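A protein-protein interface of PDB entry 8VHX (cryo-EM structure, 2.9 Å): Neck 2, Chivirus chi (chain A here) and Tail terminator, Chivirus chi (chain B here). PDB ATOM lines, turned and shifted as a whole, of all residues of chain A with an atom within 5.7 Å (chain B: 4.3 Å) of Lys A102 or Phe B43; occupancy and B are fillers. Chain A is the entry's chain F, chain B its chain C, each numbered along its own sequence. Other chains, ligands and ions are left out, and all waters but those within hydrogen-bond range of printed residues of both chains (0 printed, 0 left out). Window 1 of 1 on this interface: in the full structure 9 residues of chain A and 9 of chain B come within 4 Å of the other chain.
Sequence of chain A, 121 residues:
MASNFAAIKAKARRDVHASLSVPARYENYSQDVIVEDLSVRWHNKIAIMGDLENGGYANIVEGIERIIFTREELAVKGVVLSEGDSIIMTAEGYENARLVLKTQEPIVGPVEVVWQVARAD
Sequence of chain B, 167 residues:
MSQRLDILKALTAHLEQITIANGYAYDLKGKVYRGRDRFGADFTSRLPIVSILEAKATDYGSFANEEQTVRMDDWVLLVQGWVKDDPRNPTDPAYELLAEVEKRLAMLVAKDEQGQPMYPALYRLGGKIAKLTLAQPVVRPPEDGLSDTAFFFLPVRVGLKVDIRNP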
ATOM      1  N   GLU A  83     -11.661  -0.195  27.741  1.00  0.00           N
ATOM      2  CA  GLU A  83     -12.510  -1.349  27.504  1.00  0.00           C
ATOM      3  C   GLU A  83     -12.099  -2.495  28.414  1.00  0.00           C
ATOM      4  O   GLU A  83     -10.912  -2.736  28.645  1.00  0.00           O
ATOM      5  CB  GLU A  83     -12.424  -1.768  26.041  1.00  0.00           C
ATOM      6  CG  GLU A  83     -13.246  -2.978  25.689  1.00  0.00           C
ATOM      7  CD  GLU A  83     -12.890  -3.555  24.339  1.00  0.00           C
ATOM      8  OE1 GLU A  83     -11.683  -3.623  24.024  1.00  0.00           O
ATOM      9  OE2 GLU A  83     -13.812  -3.945  23.593  1.00  0.00           O
ATOM     10  N   GLY A  84     -13.094  -3.206  28.928  1.00  0.00           N
ATOM     11  CA  GLY A  84     -12.864  -4.290  29.843  1.00  0.00           C
ATOM     12  C   GLY A  84     -12.765  -3.897  31.292  1.00  0.00           C
ATOM     13  O   GLY A  84     -12.928  -4.761  32.159  1.00  0.00           O
ATOM     14  N   VAL A 100     -19.000  -3.749  33.202  1.00  0.00           N
ATOM     15  CA  VAL A 100     -17.836  -3.863  32.342  1.00  0.00           C
ATOM     16  C   VAL A 100     -17.919  -2.810  31.255  1.00  0.00           C
ATOM     17  O   VAL A 100     -18.851  -2.811  30.446  1.00  0.00           O
ATOM     18  CB  VAL A 100     -17.751  -5.270  31.740  1.00  0.00           C
ATOM     19  CG1 VAL A 100     -16.602  -5.364  30.830  1.00  0.00           C
ATOM     20  CG2 VAL A 100     -17.622  -6.291  32.817  1.00  0.00           C
ATOM     21  N   LEU A 101     -16.938  -1.920  31.227  1.00  0.00           N
ATOM     22  CA  LEU A 101     -16.890  -0.874  30.220  1.00  0.00           C
ATOM     23  C   LEU A 101     -16.643  -1.476  28.849  1.00  0.00           C
ATOM     24  O   LEU A 101     -15.674  -2.211  28.648  1.00  0.00           O
ATOM     25  CB  LEU A 101     -15.803   0.129  30.553  1.00  0.00           C
ATOM     26  CG  LEU A 101     -15.852   0.781  31.915  1.00  0.00           C
ATOM     27  CD1 LEU A 101     -14.902   1.879  31.882  1.00  0.00           C
ATOM     28  CD2 LEU A 101     -17.193   1.302  32.219  1.00  0.00           C
ATOM     29  N   LYS A 102     -17.518  -1.153  27.904  1.00  0.00           N
ATOM     30  CA  LYS A 102     -17.473  -1.709  26.565  1.00  0.00           C
ATOM     31  C   LYS A 102     -16.959  -0.711  25.541  1.00  0.00           C
ATOM     32  O   LYS A 102     -16.029  -1.008  24.791  1.00  0.00           O
ATOM     33  CB  LYS A 102     -18.864  -2.189  26.158  1.00  0.00           C
ATOM     34  CG  LYS A 102     -19.428  -3.302  26.998  1.00  0.00           C
ATOM     35  CD  LYS A 102     -18.605  -4.548  26.958  1.00  0.00           C
ATOM     36  CE  LYS A 102     -18.532  -5.121  25.586  1.00  0.00           C
ATOM     37  NZ  LYS A 102     -17.795  -6.379  25.595  1.00  0.00           N
ATOM     38  N   THR A 103     -17.561   0.470  25.494  1.00  0.00           N
ATOM     39  CA  THR A 103     -17.172   1.490  24.540  1.00  0.00           C
ATOM     40  C   THR A 103     -17.703   2.824  25.030  1.00  0.00           C
ATOM     41  O   THR A 103     -18.714   2.895  25.729  1.00  0.00           O
ATOM     42  CB  THR A 103     -17.684   1.176  23.127  1.00  0.00           C
ATOM     43  OG1 THR A 103     -17.031   2.027  22.180  1.00  0.00           O
ATOM     44  CG2 THR A 103     -19.167   1.396  23.024  1.00  0.00           C
ATOM     45  N   GLN A 104     -16.993   3.874  24.658  1.00  0.00           N
ATOM     46  CA  GLN A 104     -17.258   5.216  25.134  1.00  0.00           C
ATOM     47  C   GLN A 104     -18.106   5.994  24.150  1.00  0.00           C
ATOM     48  O   GLN A 104     -17.930   5.890  22.934  1.00  0.00           O
ATOM     49  CB  GLN A 104     -15.940   5.936  25.373  1.00  0.00           C
ATOM     50  CG  GLN A 104     -16.026   7.235  26.081  1.00  0.00           C
ATOM     51  CD  GLN A 104     -14.828   8.092  25.803  1.00  0.00           C
ATOM     52  OE1 GLN A 104     -13.714   7.778  26.211  1.00  0.00           O
ATOM     53  NE2 GLN A 104     -15.039   9.171  25.090  1.00  0.00           N
ATOM     54  N   TRP A 115     -19.912   6.234  29.329  1.00  0.00           N
ATOM     55  CA  TRP A 115     -19.476   4.942  28.846  1.00  0.00           C
ATOM     56  C   TRP A 115     -20.659   3.999  28.788  1.00  0.00           C
ATOM     57  O   TRP A 115     -21.440   3.915  29.739  1.00  0.00           O
ATOM     58  CB  TRP A 115     -18.394   4.361  29.740  1.00  0.00           C
ATOM     59  CG  TRP A 115     -17.062   4.922  29.501  1.00  0.00           C
ATOM     60  CD1 TRP A 115     -16.599   6.124  29.907  1.00  0.00           C
ATOM     61  CD2 TRP A 115     -16.000   4.304  28.786  1.00  0.00           C
ATOM     62  NE1 TRP A 115     -15.313   6.299  29.495  1.00  0.00           N
ATOM     63  CE2 TRP A 115     -14.921   5.189  28.802  1.00  0.00           C
ATOM     64  CE3 TRP A 115     -15.856   3.084  28.135  1.00  0.00           C
ATOM     65  CZ2 TRP A 115     -13.717   4.897  28.190  1.00  0.00           C
ATOM     66  CZ3 TRP A 115     -14.672   2.800  27.534  1.00  0.00           C
ATOM     67  CH2 TRP A 115     -13.617   3.698  27.560  1.00  0.00           C
ATOM     68  N   GLN A 116     -20.793   3.302  27.670  1.00  0.00           N
ATOM     69  CA  GLN A 116     -21.732   2.208  27.568  1.00  0.00           C
ATOM     70  C   GLN A 116     -21.093   0.967  28.163  1.00  0.00           C
ATOM     71  O   GLN A 116     -19.957   0.621  27.833  1.00  0.00           O
ATOM     72  CB  GLN A 116     -22.102   1.972  26.113  1.00  0.00           C
ATOM     73  CG  GLN A 116     -22.624   3.179  25.415  1.00  0.00           C
ATOM     74  CD  GLN A 116     -23.160   2.880  24.049  1.00  0.00           C
ATOM     75  OE1 GLN A 116     -22.963   1.795  23.515  1.00  0.00           O
ATOM     76  NE2 GLN A 116     -23.837   3.847  23.464  1.00  0.00           N
ATOM     77  N   VAL A 117     -21.824   0.292  29.045  1.00  0.00           N
ATOM     78  CA  VAL A 117     -21.260  -0.780  29.844  1.00  0.00           C
ATOM     79  C   VAL A 117     -22.172  -1.992  29.769  1.00  0.00           C
ATOM     80  O   VAL A 117     -23.235  -1.967  29.152  1.00  0.00           O
ATOM     81  CB  VAL A 117     -21.041  -0.370  31.309  1.00  0.00           C
ATOM     82  CG1 VAL A 117     -20.278   0.893  31.378  1.00  0.00           C
ATOM     83  CG2 VAL A 117     -22.323  -0.243  32.020  1.00  0.00           C
ATOM     84  N   ALA A 118     -21.718  -3.069  30.395  1.00  0.00           N
ATOM     85  CA  ALA A 118     -22.438  -4.326  30.424  1.00  0.00           C
ATOM     86  C   ALA A 118     -22.391  -4.918  31.818  1.00  0.00           C
ATOM     87  O   ALA A 118     -21.312  -5.093  32.388  1.00  0.00           O
ATOM     88  CB  ALA A 118     -21.843  -5.303  29.428  1.00  0.00           C
ATOM     89  N   TYR B  33      -9.482  -5.566  15.750  1.00  0.00           N
ATOM     90  CA  TYR B  33     -10.370  -5.970  16.816  1.00  0.00           C
ATOM     91  C   TYR B  33     -11.334  -7.039  16.328  1.00  0.00           C
ATOM     92  O   TYR B  33     -11.429  -7.339  15.140  1.00  0.00           O
ATOM     93  CB  TYR B  33     -11.110  -4.759  17.351  1.00  0.00           C
ATOM     94  CG  TYR B  33     -10.214  -3.795  18.063  1.00  0.00           C
ATOM     95  CD1 TYR B  33      -9.615  -4.135  19.251  1.00  0.00           C
ATOM     96  CD2 TYR B  33      -9.952  -2.555  17.539  1.00  0.00           C
ATOM     97  CE1 TYR B  33      -8.797  -3.265  19.902  1.00  0.00           C
ATOM     98  CE2 TYR B  33      -9.131  -1.678  18.183  1.00  0.00           C
ATOM     99  CZ  TYR B  33      -8.552  -2.036  19.365  1.00  0.00           C
ATOM    100  OH  TYR B  33      -7.727  -1.152  20.017  1.00  0.00           O
ATOM    101  N   PHE B  39     -18.218   0.154  18.213  1.00  0.00           N
ATOM    102  CA  PHE B  39     -16.927   0.796  18.409  1.00  0.00           C
ATOM    103  C   PHE B  39     -17.171   2.274  18.674  1.00  0.00           C
ATOM    104  O   PHE B  39     -17.681   2.985  17.804  1.00  0.00           O
ATOM    105  CB  PHE B  39     -16.033   0.615  17.190  1.00  0.00           C
ATOM    106  CG  PHE B  39     -15.671  -0.798  16.898  1.00  0.00           C
ATOM    107  CD1 PHE B  39     -16.473  -1.575  16.111  1.00  0.00           C
ATOM    108  CD2 PHE B  39     -14.519  -1.345  17.391  1.00  0.00           C
ATOM    109  CE1 PHE B  39     -16.142  -2.856  15.838  1.00  0.00           C
ATOM    110  CE2 PHE B  39     -14.195  -2.628  17.117  1.00  0.00           C
ATOM    111  CZ  PHE B  39     -15.002  -3.380  16.341  1.00  0.00           C
ATOM    112  N   GLY B  40     -16.806   2.737  19.859  1.00  0.00           N
ATOM    113  CA  GLY B  40     -17.004   4.109  20.251  1.00  0.00           C
ATOM    114  C   GLY B  40     -15.745   4.942  20.209  1.00  0.00           C
ATOM    115  O   GLY B  40     -14.786   4.636  19.494  1.00  0.00           O
ATOM    116  N   ALA B  41     -15.749   6.015  20.995  1.00  0.00           N
ATOM    117  CA  ALA B  41     -14.680   7.000  20.946  1.00  0.00           C
ATOM    118  C   ALA B  41     -13.351   6.456  21.429  1.00  0.00           C
ATOM    119  O   ALA B  41     -12.306   7.016  21.086  1.00  0.00           O
ATOM    120  CB  ALA B  41     -15.060   8.207  21.776  1.00  0.00           C
ATOM    121  N   ASP B  42     -13.394   5.387  22.205  1.00  0.00           N
ATOM    122  CA  ASP B  42     -12.177   4.759  22.667  1.00  0.00           C
ATOM    123  C   ASP B  42     -11.488   4.121  21.487  1.00  0.00           C
ATOM    124  O   ASP B  42     -10.281   3.904  21.511  1.00  0.00           O
ATOM    125  CB  ASP B  42     -12.494   3.713  23.735  1.00  0.00           C
ATOM    126  CG  ASP B  42     -13.764   2.928  23.447  1.00  0.00           C
ATOM    127  OD1 ASP B  42     -14.776   3.521  23.023  1.00  0.00           O
ATOM    128  OD2 ASP B  42     -13.753   1.702  23.672  1.00  0.00           O
ATOM    129  N   PHE B  43     -12.253   3.822  20.447  1.00  0.00           N
ATOM    130  CA  PHE B  43     -11.700   3.182  19.270  1.00  0.00           C
ATOM    131  C   PHE B  43     -11.541   4.189  18.164  1.00  0.00           C
ATOM    132  O   PHE B  43     -10.455   4.371  17.636  1.00  0.00           O
ATOM    133  CB  PHE B  43     -12.635   2.086  18.789  1.00  0.00           C
ATOM    134  CG  PHE B  43     -12.802   0.954  19.751  1.00  0.00           C
ATOM    135  CD1 PHE B  43     -11.818  -0.006  19.885  1.00  0.00           C
ATOM    136  CD2 PHE B  43     -13.956   0.836  20.502  1.00  0.00           C
ATOM    137  CE1 PHE B  43     -11.973  -1.058  20.762  1.00  0.00           C
ATOM    138  CE2 PHE B  43     -14.120  -0.216  21.380  1.00  0.00           C
ATOM    139  CZ  PHE B  43     -13.126  -1.164  21.513  1.00  0.00           C
ATOM    140  N   THR B  44     -12.629   4.849  17.804  1.00  0.00           N
ATOM    141  CA  THR B  44     -12.595   5.819  16.721  1.00  0.00           C
ATOM    142  C   THR B  44     -11.552   6.904  16.928  1.00  0.00           C
ATOM    143  O   THR B  44     -11.188   7.599  15.987  1.00  0.00           O
ATOM    144  CB  THR B  44     -13.966   6.487  16.549  1.00  0.00           C
ATOM    145  OG1 THR B  44     -14.243   7.307  17.690  1.00  0.00           O
ATOM    146  CG2 THR B  44     -15.050   5.435  16.415  1.00  0.00           C
ATOM    147  N   SER B  45     -11.077   7.066  18.150  1.00  0.00           N
ATOM    148  CA  SER B  45     -10.039   8.040  18.409  1.00  0.00           C
ATOM    149  C   SER B  45      -8.695   7.442  18.093  1.00  0.00           C
ATOM    150  O   SER B  45      -7.667   8.009  18.446  1.00  0.00           O
ATOM    151  CB  SER B  45     -10.062   8.451  19.868  1.00  0.00           C
ATOM    152  OG  SER B  45      -9.717   7.361  20.703  1.00  0.00           O
ATOM    153  N   ARG B  46      -8.687   6.298  17.430  1.00  0.00           N
ATOM    154  CA  ARG B  46      -7.431   5.611  17.163  1.00  0.00           C
ATOM    155  C   ARG B  46      -7.417   4.954  15.789  1.00  0.00           C
ATOM    156  O   ARG B  46      -6.734   3.943  15.609  1.00  0.00           O
ATOM    157  CB  ARG B  46      -7.153   4.555  18.223  1.00  0.00           C
ATOM    158  CG  ARG B  46      -7.029   5.102  19.621  1.00  0.00           C
ATOM    159  CD  ARG B  46      -6.692   4.010  20.601  1.00  0.00           C
ATOM    160  NE  ARG B  46      -7.743   3.007  20.672  1.00  0.00           N
ATOM    161  CZ  ARG B  46      -7.604   1.758  20.250  1.00  0.00           C
ATOM    162  NH1 ARG B  46      -6.454   1.360  19.731  1.00  0.00           N
ATOM    163  NH2 ARG B  46      -8.609   0.907  20.353  1.00  0.00           N
ATOM    164  N   LEU B  47      -8.154   5.493  14.829  1.00  0.00           N
ATOM    165  CA  LEU B  47      -8.215   4.901  13.502  1.00  0.00           C
ATOM    166  C   LEU B  47      -6.831   4.917  12.854  1.00  0.00           C
ATOM    167  O   LEU B  47      -5.988   5.746  13.216  1.00  0.00           O
ATOM    168  CB  LEU B  47      -9.215   5.669  12.645  1.00  0.00           C
ATOM    169  CG  LEU B  47     -10.586   5.774  13.294  1.00  0.00           C
ATOM    170  CD1 LEU B  47     -11.415   6.810  12.593  1.00  0.00           C
ATOM    171  CD2 LEU B  47     -11.269   4.436  13.256  1.00  0.00           C
ATOM    172  N   ILE B  49      -8.827   1.187  12.055  1.00  0.00           N
ATOM    173  CA  ILE B  49      -9.182   0.019  12.843  1.00  0.00           C
ATOM    174  C   ILE B  49      -9.905  -0.962  11.942  1.00  0.00           C
ATOM    175  O   ILE B  49     -10.807  -0.576  11.195  1.00  0.00           O
ATOM    176  CB  ILE B  49     -10.058   0.399  14.055  1.00  0.00           C
ATOM    177  CG1 ILE B  49      -9.203   1.026  15.147  1.00  0.00           C
ATOM    178  CG2 ILE B  49     -10.805  -0.797  14.591  1.00  0.00           C
ATOM    179  CD1 ILE B  49      -9.997   1.516  16.302  1.00  0.00           C
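The backbone carbonyl oxygen (O) of Gly B40 sits close to the side-chain hydroxyl (OG1) of Thr B44 (3.3 Å).
O of Ala B41 sits at hydrogen-bond distance from OG of Ser B45 (2.6 Å).
The backbone carbonyl oxygen (O) of Asp B42 sits at hydrogen-bond distance from the guanidinium group (NE) of Arg B46.
The backbone NH (N) of Lys A102 sits at hydrogen-bond distance from the backbone carbonyl oxygen (O) of Gln A116.
O of Thr A103 is in hydrogen-bond range of N of Gln A116, 2.9 Å away.
The side-chain hydroxyl (OG1) of Thr A103 sits at hydrogen-bond distance from the backbone NH (N) of Gly B40, at 2.4 Å.
O of Gln A104 lies within hydrogen-bond range of N of Ala B41, 2.9 Å away.
The side-chain hydroxyl (OG1) of Thr A103 lies within hydrogen-bond range of the side-chain carboxylate (OD1) of Asp B42.
The side-chain carboxylate (OD1) of Asp B42 is in hydrogen-bond range of the backbone NH (N) of Gln A104, 2.8 Å away.
Hydrophobic or aromatic side chains of chain A within 4 Å of the printed part of chain B: Trp A115.
Hydrophobic or aromatic side chains of chain B within 4 Å of the printed part of chain A: Ala B41 and Phe B43.
Along chain B the printed residues that touch a printed residue of chain A span positions 39 to 43.
Among the printed residues, no Asp or Glu carboxylate lies within 4 Å of a Lys or Arg side-chain nitrogen of the other chain.
Of the printed residues of chain B, Glu A83 touches Phe B43.
Of the printed residues of chain B, Lys A102 touches Asp B42 (3.7 Å) and Phe B43 (3.99 Å).
Of the printed residues of chain B, Gln A104 touches Gly B40, Ala B41 and Asp B42.
Of the printed residues of chain B, Trp A115 touches Asp B42 (3.99 Å).
Gln A116 touches none of the printed residues of chain B.
Printed residues of chain A within 4 Å of Phe B39: Thr A103.
Printed residues of chain A within 4 Å of Ala B41: Gln A104.
Of the printed residues of chain A, Phe B43 touches Glu A83, Lys A102 and Thr A103.
Leu B47 touches none of the printed residues of chain A.
Among the printed residues, pairs that only touch across the chains: Gln A104 with Gly B40 (3.4 Å), Thr A103 with Phe B39 (3.5 Å), Glu A83 with Phe B43 (3.5 Å), Thr A103 with Phe B43 (3.7 Å), Lys A102 with Asp B42 (3.7 Å), Trp A115 with Asp B42 (3.99 Å) and Lys A102 with Phe B43 (3.99 Å).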
